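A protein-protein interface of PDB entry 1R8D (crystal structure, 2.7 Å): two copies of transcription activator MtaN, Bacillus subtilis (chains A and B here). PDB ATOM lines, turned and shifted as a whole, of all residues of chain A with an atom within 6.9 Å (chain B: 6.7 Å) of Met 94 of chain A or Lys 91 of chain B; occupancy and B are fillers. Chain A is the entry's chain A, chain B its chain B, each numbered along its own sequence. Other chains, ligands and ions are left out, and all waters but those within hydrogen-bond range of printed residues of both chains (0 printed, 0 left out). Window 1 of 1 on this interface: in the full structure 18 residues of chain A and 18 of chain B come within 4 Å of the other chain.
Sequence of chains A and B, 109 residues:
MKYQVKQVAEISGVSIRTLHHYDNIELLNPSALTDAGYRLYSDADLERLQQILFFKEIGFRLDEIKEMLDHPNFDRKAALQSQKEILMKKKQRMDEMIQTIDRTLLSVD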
ATOM      1  N   LYS A  89      -4.003  30.293   4.941  1.00  0.00           N
ATOM      2  CA  LYS A  89      -4.865  31.142   4.131  1.00  0.00           C
ATOM      3  C   LYS A  89      -4.624  30.922   2.645  1.00  0.00           C
ATOM      4  O   LYS A  89      -5.574  30.885   1.862  1.00  0.00           O
ATOM      5  CB  LYS A  89      -4.668  32.613   4.481  1.00  0.00           C
ATOM      6  CG  LYS A  89      -5.371  33.027   5.756  1.00  0.00           C
ATOM      7  CD  LYS A  89      -5.294  34.531   5.980  1.00  0.00           C
ATOM      8  CE  LYS A  89      -6.035  34.926   7.247  1.00  0.00           C
ATOM      9  NZ  LYS A  89      -5.516  34.197   8.445  1.00  0.00           N
ATOM     10  N   LYS A  90      -3.360  30.781   2.250  1.00  0.00           N
ATOM     11  CA  LYS A  90      -3.048  30.556   0.845  1.00  0.00           C
ATOM     12  C   LYS A  90      -3.763  29.292   0.398  1.00  0.00           C
ATOM     13  O   LYS A  90      -4.267  29.207  -0.724  1.00  0.00           O
ATOM     14  CB  LYS A  90      -1.545  30.394   0.638  1.00  0.00           C
ATOM     15  CG  LYS A  90      -0.753  31.693   0.632  1.00  0.00           C
ATOM     16  CD  LYS A  90       0.688  31.420   0.208  1.00  0.00           C
ATOM     17  CE  LYS A  90       1.490  32.697   0.011  1.00  0.00           C
ATOM     18  NZ  LYS A  90       2.878  32.389  -0.453  1.00  0.00           N
ATOM     19  N   LYS A  91      -3.811  28.313   1.296  1.00  0.00           N
ATOM     20  CA  LYS A  91      -4.474  27.044   1.018  1.00  0.00           C
ATOM     21  C   LYS A  91      -5.983  27.268   0.872  1.00  0.00           C
ATOM     22  O   LYS A  91      -6.627  26.693  -0.010  1.00  0.00           O
ATOM     23  CB  LYS A  91      -4.192  26.057   2.154  1.00  0.00           C
ATOM     24  CG  LYS A  91      -4.872  24.706   2.003  1.00  0.00           C
ATOM     25  CD  LYS A  91      -4.631  23.829   3.225  1.00  0.00           C
ATOM     26  CE  LYS A  91      -5.257  22.453   3.058  1.00  0.00           C
ATOM     27  NZ  LYS A  91      -4.990  21.597   4.246  1.00  0.00           N
ATOM     28  N   GLN A  92      -6.537  28.118   1.734  1.00  0.00           N
ATOM     29  CA  GLN A  92      -7.965  28.422   1.710  1.00  0.00           C
ATOM     30  C   GLN A  92      -8.349  29.100   0.395  1.00  0.00           C
ATOM     31  O   GLN A  92      -9.420  28.839  -0.157  1.00  0.00           O
ATOM     32  CB  GLN A  92      -8.322  29.326   2.899  1.00  0.00           C
ATOM     33  CG  GLN A  92      -9.817  29.566   3.109  1.00  0.00           C
ATOM     34  CD  GLN A  92     -10.114  30.519   4.272  1.00  0.00           C
ATOM     35  OE1 GLN A  92     -11.274  30.760   4.608  1.00  0.00           O
ATOM     36  NE2 GLN A  92      -9.064  31.063   4.885  1.00  0.00           N
ATOM     37  N   ARG A  93      -7.469  29.965  -0.106  1.00  0.00           N
ATOM     38  CA  ARG A  93      -7.725  30.663  -1.357  1.00  0.00           C
ATOM     39  C   ARG A  93      -7.815  29.641  -2.487  1.00  0.00           C
ATOM     40  O   ARG A  93      -8.763  29.636  -3.270  1.00  0.00           O
ATOM     41  CB  ARG A  93      -6.618  31.668  -1.638  1.00  0.00           C
ATOM     42  N   MET A  94      -6.832  28.756  -2.555  1.00  0.00           N
ATOM     43  CA  MET A  94      -6.819  27.746  -3.596  1.00  0.00           C
ATOM     44  C   MET A  94      -8.071  26.885  -3.550  1.00  0.00           C
ATOM     45  O   MET A  94      -8.568  26.436  -4.586  1.00  0.00           O
ATOM     46  CB  MET A  94      -5.578  26.877  -3.458  1.00  0.00           C
ATOM     47  CG  MET A  94      -4.326  27.690  -3.317  1.00  0.00           C
ATOM     48  SD  MET A  94      -2.901  26.761  -3.808  1.00  0.00           S
ATOM     49  CE  MET A  94      -3.107  26.883  -5.577  1.00  0.00           C
ATOM     50  N   ASP A  95      -8.588  26.645  -2.352  1.00  0.00           N
ATOM     51  CA  ASP A  95      -9.796  25.845  -2.245  1.00  0.00           C
ATOM     52  C   ASP A  95     -10.927  26.544  -2.980  1.00  0.00           C
ATOM     53  O   ASP A  95     -11.545  25.960  -3.877  1.00  0.00           O
ATOM     54  CB  ASP A  95     -10.163  25.625  -0.777  1.00  0.00           C
ATOM     55  CG  ASP A  95      -9.692  24.278  -0.265  1.00  0.00           C
ATOM     56  OD1 ASP A  95      -9.285  24.201   0.921  1.00  0.00           O
ATOM     57  OD2 ASP A  95      -9.740  23.298  -1.054  1.00  0.00           O
ATOM     58  N   GLU A  96     -11.178  27.799  -2.609  1.00  0.00           N
ATOM     59  CA  GLU A  96     -12.229  28.594  -3.243  1.00  0.00           C
ATOM     60  C   GLU A  96     -12.018  28.601  -4.757  1.00  0.00           C
ATOM     61  O   GLU A  96     -12.974  28.595  -5.529  1.00  0.00           O
ATOM     62  CB  GLU A  96     -12.200  30.024  -2.701  1.00  0.00           C
ATOM     63  CG  GLU A  96     -11.907  30.076  -1.202  1.00  0.00           C
ATOM     64  CD  GLU A  96     -11.831  31.489  -0.642  1.00  0.00           C
ATOM     65  OE1 GLU A  96     -11.239  32.373  -1.307  1.00  0.00           O
ATOM     66  OE2 GLU A  96     -12.352  31.713   0.475  1.00  0.00           O
ATOM     67  N   MET A  97     -10.758  28.596  -5.179  1.00  0.00           N
ATOM     68  CA  MET A  97     -10.455  28.590  -6.602  1.00  0.00           C
ATOM     69  C   MET A  97     -10.896  27.276  -7.239  1.00  0.00           C
ATOM     70  O   MET A  97     -11.498  27.273  -8.314  1.00  0.00           O
ATOM     71  CB  MET A  97      -8.953  28.820  -6.832  1.00  0.00           C
ATOM     72  CG  MET A  97      -8.494  30.259  -6.587  1.00  0.00           C
ATOM     73  SD  MET A  97      -6.693  30.522  -6.715  1.00  0.00           S
ATOM     74  CE  MET A  97      -6.450  30.295  -8.444  1.00  0.00           C
ATOM     75  N   ILE A  98     -10.602  26.161  -6.574  1.00  0.00           N
ATOM     76  CA  ILE A  98     -10.987  24.847  -7.083  1.00  0.00           C
ATOM     77  C   ILE A  98     -12.507  24.684  -7.084  1.00  0.00           C
ATOM     78  O   ILE A  98     -13.069  24.075  -8.005  1.00  0.00           O
ATOM     79  CB  ILE A  98     -10.360  23.720  -6.254  1.00  0.00           C
ATOM     80  CG1 ILE A  98      -8.844  23.740  -6.446  1.00  0.00           C
ATOM     81  CG2 ILE A  98     -10.941  22.377  -6.671  1.00  0.00           C
ATOM     82  CD1 ILE A  98      -8.110  22.655  -5.715  1.00  0.00           C
ATOM     83  N   GLN A  99     -13.175  25.224  -6.063  1.00  0.00           N
ATOM     84  CA  GLN A  99     -14.635  25.145  -6.026  1.00  0.00           C
ATOM     85  C   GLN A  99     -15.185  25.853  -7.251  1.00  0.00           C
ATOM     86  O   GLN A  99     -16.006  25.297  -7.988  1.00  0.00           O
ATOM     87  CB  GLN A  99     -15.199  25.819  -4.781  1.00  0.00           C
ATOM     88  CG  GLN A  99     -15.055  25.007  -3.513  1.00  0.00           C
ATOM     89  CD  GLN A  99     -15.489  25.787  -2.285  1.00  0.00           C
ATOM     90  OE1 GLN A  99     -16.608  26.310  -2.228  1.00  0.00           O
ATOM     91  NE2 GLN A  99     -14.603  25.870  -1.293  1.00  0.00           N
ATOM     92  N   THR A 100     -14.708  27.081  -7.465  1.00  0.00           N
ATOM     93  CA  THR A 100     -15.143  27.886  -8.595  1.00  0.00           C
ATOM     94  C   THR A 100     -14.988  27.094  -9.874  1.00  0.00           C
ATOM     95  O   THR A 100     -15.827  27.194 -10.765  1.00  0.00           O
ATOM     96  CB  THR A 100     -14.337  29.196  -8.714  1.00  0.00           C
ATOM     97  OG1 THR A 100     -14.563  30.014  -7.560  1.00  0.00           O
ATOM     98  CG2 THR A 100     -14.769  29.971  -9.938  1.00  0.00           C
ATOM     99  N   ILE B  86      -3.432  21.390 -11.180  1.00  0.00           N
ATOM    100  CA  ILE B  86      -2.293  22.218 -10.790  1.00  0.00           C
ATOM    101  C   ILE B  86      -2.551  22.891  -9.451  1.00  0.00           C
ATOM    102  O   ILE B  86      -1.659  22.986  -8.601  1.00  0.00           O
ATOM    103  CB  ILE B  86      -2.029  23.307 -11.831  1.00  0.00           C
ATOM    104  CG1 ILE B  86      -1.490  22.665 -13.112  1.00  0.00           C
ATOM    105  CG2 ILE B  86      -1.080  24.355 -11.259  1.00  0.00           C
ATOM    106  CD1 ILE B  86      -1.382  23.621 -14.271  1.00  0.00           C
ATOM    107  N   LEU B  87      -3.776  23.368  -9.275  1.00  0.00           N
ATOM    108  CA  LEU B  87      -4.154  24.022  -8.038  1.00  0.00           C
ATOM    109  C   LEU B  87      -4.090  23.027  -6.892  1.00  0.00           C
ATOM    110  O   LEU B  87      -3.702  23.376  -5.773  1.00  0.00           O
ATOM    111  CB  LEU B  87      -5.568  24.588  -8.153  1.00  0.00           C
ATOM    112  CG  LEU B  87      -5.753  25.842  -9.010  1.00  0.00           C
ATOM    113  CD1 LEU B  87      -7.238  26.131  -9.183  1.00  0.00           C
ATOM    114  CD2 LEU B  87      -5.054  27.020  -8.342  1.00  0.00           C
ATOM    115  N   MET B  88      -4.469  21.783  -7.176  1.00  0.00           N
ATOM    116  CA  MET B  88      -4.460  20.740  -6.162  1.00  0.00           C
ATOM    117  C   MET B  88      -3.041  20.461  -5.687  1.00  0.00           C
ATOM    118  O   MET B  88      -2.778  20.455  -4.482  1.00  0.00           O
ATOM    119  CB  MET B  88      -5.099  19.456  -6.704  1.00  0.00           C
ATOM    120  CG  MET B  88      -6.577  19.602  -7.019  1.00  0.00           C
ATOM    121  SD  MET B  88      -7.356  18.111  -7.671  1.00  0.00           S
ATOM    122  CE  MET B  88      -8.614  17.845  -6.391  1.00  0.00           C
ATOM    123  N   LYS B  89      -2.127  20.238  -6.629  1.00  0.00           N
ATOM    124  CA  LYS B  89      -0.739  19.979  -6.270  1.00  0.00           C
ATOM    125  C   LYS B  89      -0.194  21.108  -5.389  1.00  0.00           C
ATOM    126  O   LYS B  89       0.541  20.865  -4.427  1.00  0.00           O
ATOM    127  CB  LYS B  89       0.113  19.828  -7.533  1.00  0.00           C
ATOM    128  CG  LYS B  89      -0.146  18.531  -8.303  1.00  0.00           C
ATOM    129  CD  LYS B  89       0.473  18.549  -9.714  1.00  0.00           C
ATOM    130  CE  LYS B  89       2.003  18.583  -9.704  1.00  0.00           C
ATOM    131  NZ  LYS B  89       2.620  17.318  -9.204  1.00  0.00           N
ATOM    132  N   LYS B  90      -0.564  22.343  -5.711  1.00  0.00           N
ATOM    133  CA  LYS B  90      -0.102  23.483  -4.936  1.00  0.00           C
ATOM    134  C   LYS B  90      -0.606  23.360  -3.513  1.00  0.00           C
ATOM    135  O   LYS B  90       0.116  23.648  -2.560  1.00  0.00           O
ATOM    136  CB  LYS B  90      -0.600  24.793  -5.551  1.00  0.00           C
ATOM    137  CG  LYS B  90       0.157  25.231  -6.797  1.00  0.00           C
ATOM    138  CD  LYS B  90      -0.160  26.682  -7.148  1.00  0.00           C
ATOM    139  CE  LYS B  90       0.686  27.192  -8.313  1.00  0.00           C
ATOM    140  NZ  LYS B  90       0.335  28.596  -8.694  1.00  0.00           N
ATOM    141  N   LYS B  91      -1.858  22.929  -3.389  1.00  0.00           N
ATOM    142  CA  LYS B  91      -2.522  22.734  -2.099  1.00  0.00           C
ATOM    143  C   LYS B  91      -1.683  21.738  -1.284  1.00  0.00           C
ATOM    144  O   LYS B  91      -1.331  21.975  -0.120  1.00  0.00           O
ATOM    145  CB  LYS B  91      -3.924  22.166  -2.354  1.00  0.00           C
ATOM    146  CG  LYS B  91      -4.899  22.186  -1.178  1.00  0.00           C
ATOM    147  CD  LYS B  91      -6.112  21.288  -1.463  1.00  0.00           C
ATOM    148  CE  LYS B  91      -7.330  21.703  -0.653  1.00  0.00           C
ATOM    149  NZ  LYS B  91      -7.026  21.866   0.801  1.00  0.00           N
ATOM    150  N   GLN B  92      -1.364  20.622  -1.929  1.00  0.00           N
ATOM    151  CA  GLN B  92      -0.575  19.552  -1.340  1.00  0.00           C
ATOM    152  C   GLN B  92       0.769  20.075  -0.807  1.00  0.00           C
ATOM    153  O   GLN B  92       1.139  19.803   0.342  1.00  0.00           O
ATOM    154  CB  GLN B  92      -0.345  18.483  -2.404  1.00  0.00           C
ATOM    155  CG  GLN B  92       0.075  17.125  -1.897  1.00  0.00           C
ATOM    156  CD  GLN B  92       0.536  16.226  -3.034  1.00  0.00           C
ATOM    157  OE1 GLN B  92       1.640  16.389  -3.560  1.00  0.00           O
ATOM    158  NE2 GLN B  92      -0.317  15.286  -3.433  1.00  0.00           N
ATOM    159  N   ARG B  93       1.499  20.818  -1.643  1.00  0.00           N
ATOM    160  CA  ARG B  93       2.789  21.369  -1.229  1.00  0.00           C
ATOM    161  C   ARG B  93       2.571  22.256  -0.001  1.00  0.00           C
ATOM    162  O   ARG B  93       3.355  22.236   0.945  1.00  0.00           O
ATOM    163  CB  ARG B  93       3.420  22.166  -2.372  1.00  0.00           C
ATOM    164  N   MET B  94       1.488  23.022  -0.021  1.00  0.00           N
ATOM    165  CA  MET B  94       1.140  23.888   1.099  1.00  0.00           C
ATOM    166  C   MET B  94       1.000  23.019   2.345  1.00  0.00           C
ATOM    167  O   MET B  94       1.483  23.365   3.426  1.00  0.00           O
ATOM    168  CB  MET B  94      -0.193  24.573   0.828  1.00  0.00           C
ATOM    169  CG  MET B  94      -0.200  25.511  -0.348  1.00  0.00           C
ATOM    170  SD  MET B  94       0.267  27.137   0.181  1.00  0.00           S
ATOM    171  CE  MET B  94       2.029  27.051  -0.027  1.00  0.00           C
ATOM    172  N   ASP B  95       0.320  21.888   2.188  1.00  0.00           N
ATOM    173  CA  ASP B  95       0.123  20.976   3.306  1.00  0.00           C
ATOM    174  C   ASP B  95       1.436  20.458   3.871  1.00  0.00           C
ATOM    175  O   ASP B  95       1.684  20.570   5.075  1.00  0.00           O
ATOM    176  CB  ASP B  95      -0.760  19.791   2.898  1.00  0.00           C
ATOM    177  CG  ASP B  95      -2.241  20.071   3.101  1.00  0.00           C
ATOM    178  OD1 ASP B  95      -2.615  20.517   4.216  1.00  0.00           O
ATOM    179  OD2 ASP B  95      -3.028  19.837   2.150  1.00  0.00           O
ATOM    180  N   GLU B  96       2.278  19.893   3.012  1.00  0.00           N
ATOM    181  CA  GLU B  96       3.562  19.376   3.476  1.00  0.00           C
ATOM    182  C   GLU B  96       4.323  20.450   4.275  1.00  0.00           C
ATOM    183  O   GLU B  96       4.887  20.162   5.333  1.00  0.00           O
ATOM    184  CB  GLU B  96       4.403  18.904   2.289  1.00  0.00           C
ATOM    185  CG  GLU B  96       3.583  18.206   1.203  1.00  0.00           C
ATOM    186  CD  GLU B  96       4.437  17.673   0.059  1.00  0.00           C
ATOM    187  OE1 GLU B  96       5.375  18.380  -0.371  1.00  0.00           O
ATOM    188  OE2 GLU B  96       4.163  16.551  -0.419  1.00  0.00           O
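Of the printed residues of chain B, Met 94 of chain A touches Leu 87 (3.4 Å), Lys 90 (3.3 Å) and Lys 91 (3.99 Å).
Printed residues of chain A within 4 Å of Lys 91 of chain B: Lys 91 (2.9 Å), Met 94 (3.99 Å) and Asp 95 (2.9 Å).
Of the printed residues of chain B, Asp 95 of chain A touches Lys 91 (2.9 Å).
Printed residues of chain A within 4 Å of Asp 95 of chain B: Lys 91.
Of the printed residues of chain A, Leu 87 of chain B touches Met 94 (3.4 Å), Met 97 (3.6 Å) and Ile 98 (3.8 Å).
Arg 93 of chain B touches none of the printed residues of chain A.
The nearest printed residue of chain A that does not touch Lys 91 of chain B is Ile 98 of chain A (4.9 Å).
The nearest printed residue of chain B that does not touch Asp 95 of chain A is Leu 87 of chain B (6.8 Å).
CB of Lys 90 of chain A touches SD of Met 94 of chain B, 3.8 Å away.
Lys 91 of chain A touches Lys 91 of chain B (CE to NZ, 2.9 Å).
CE of Met 94 of chain A touches CD2 of Leu 87 of chain B, 3.4 Å away.
CB of Lys 90 of chain B touches CE of Met 94 of chain A, at 3.3 Å.
Met 94 of chain A touches Lys 91 of chain B (SD to N, 3.99 Å).
Leu 87 of chain B touches Met 97 of chain A.
Ile 98 of chain A touches Leu 87 of chain B.
Met 88 of chain B touches Ile 98 of chain A (CG to CD1, 3.7 Å).
Of the 12 printed residues of chain A, 6 touch a printed residue of chain B.
Printed residues of chain A that touch a printed residue of chain B: Lys 90, Lys 91, Met 94, Asp 95, Met 97 and Ile 98.
Along chain A the printed residues that touch a printed residue of chain B span positions 90 to 98.
Of the 11 printed residues of chain B, 6 touch a printed residue of chain A.
Hydrophobic or aromatic side chains of chain B within 4 Å of the printed part of chain A: Leu 87, Met 88 and Met 94.
Lys 90 of chain A touches Met 94 of chain B, and with the chains exchanged Met 94 of chain A touches Lys 90 of chain B.
Lys 91 of chain B touches its own counterpart, Lys 91 of chain A.
Lys 91 of chain A touches Asp 95 of chain B, and with the chains exchanged Asp 95 of chain A touches Lys 91 of chain B.
Met 94 of chain A touches Lys 91 of chain B, but with the chains exchanged Lys 91 of chain A does not touch Met 94 of chain B (4.4 Å).
Positions printed for both chains: 89, 90, 91, 92, 93, 94, 95 and 96.
Of the 10 pairs that touch across the chains among the printed residues, 5 have their exchanged pair printed and touching as well.
NZ of Lys 91 of chain A lies within salt-bridge range of OD1 of Asp 95 of chain B (2.6 Å).
The side-chain carboxylate of Asp 95 of chain A is in salt-bridge range of the side-chain amino group of Lys 91 of chain B (3.3 Å).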
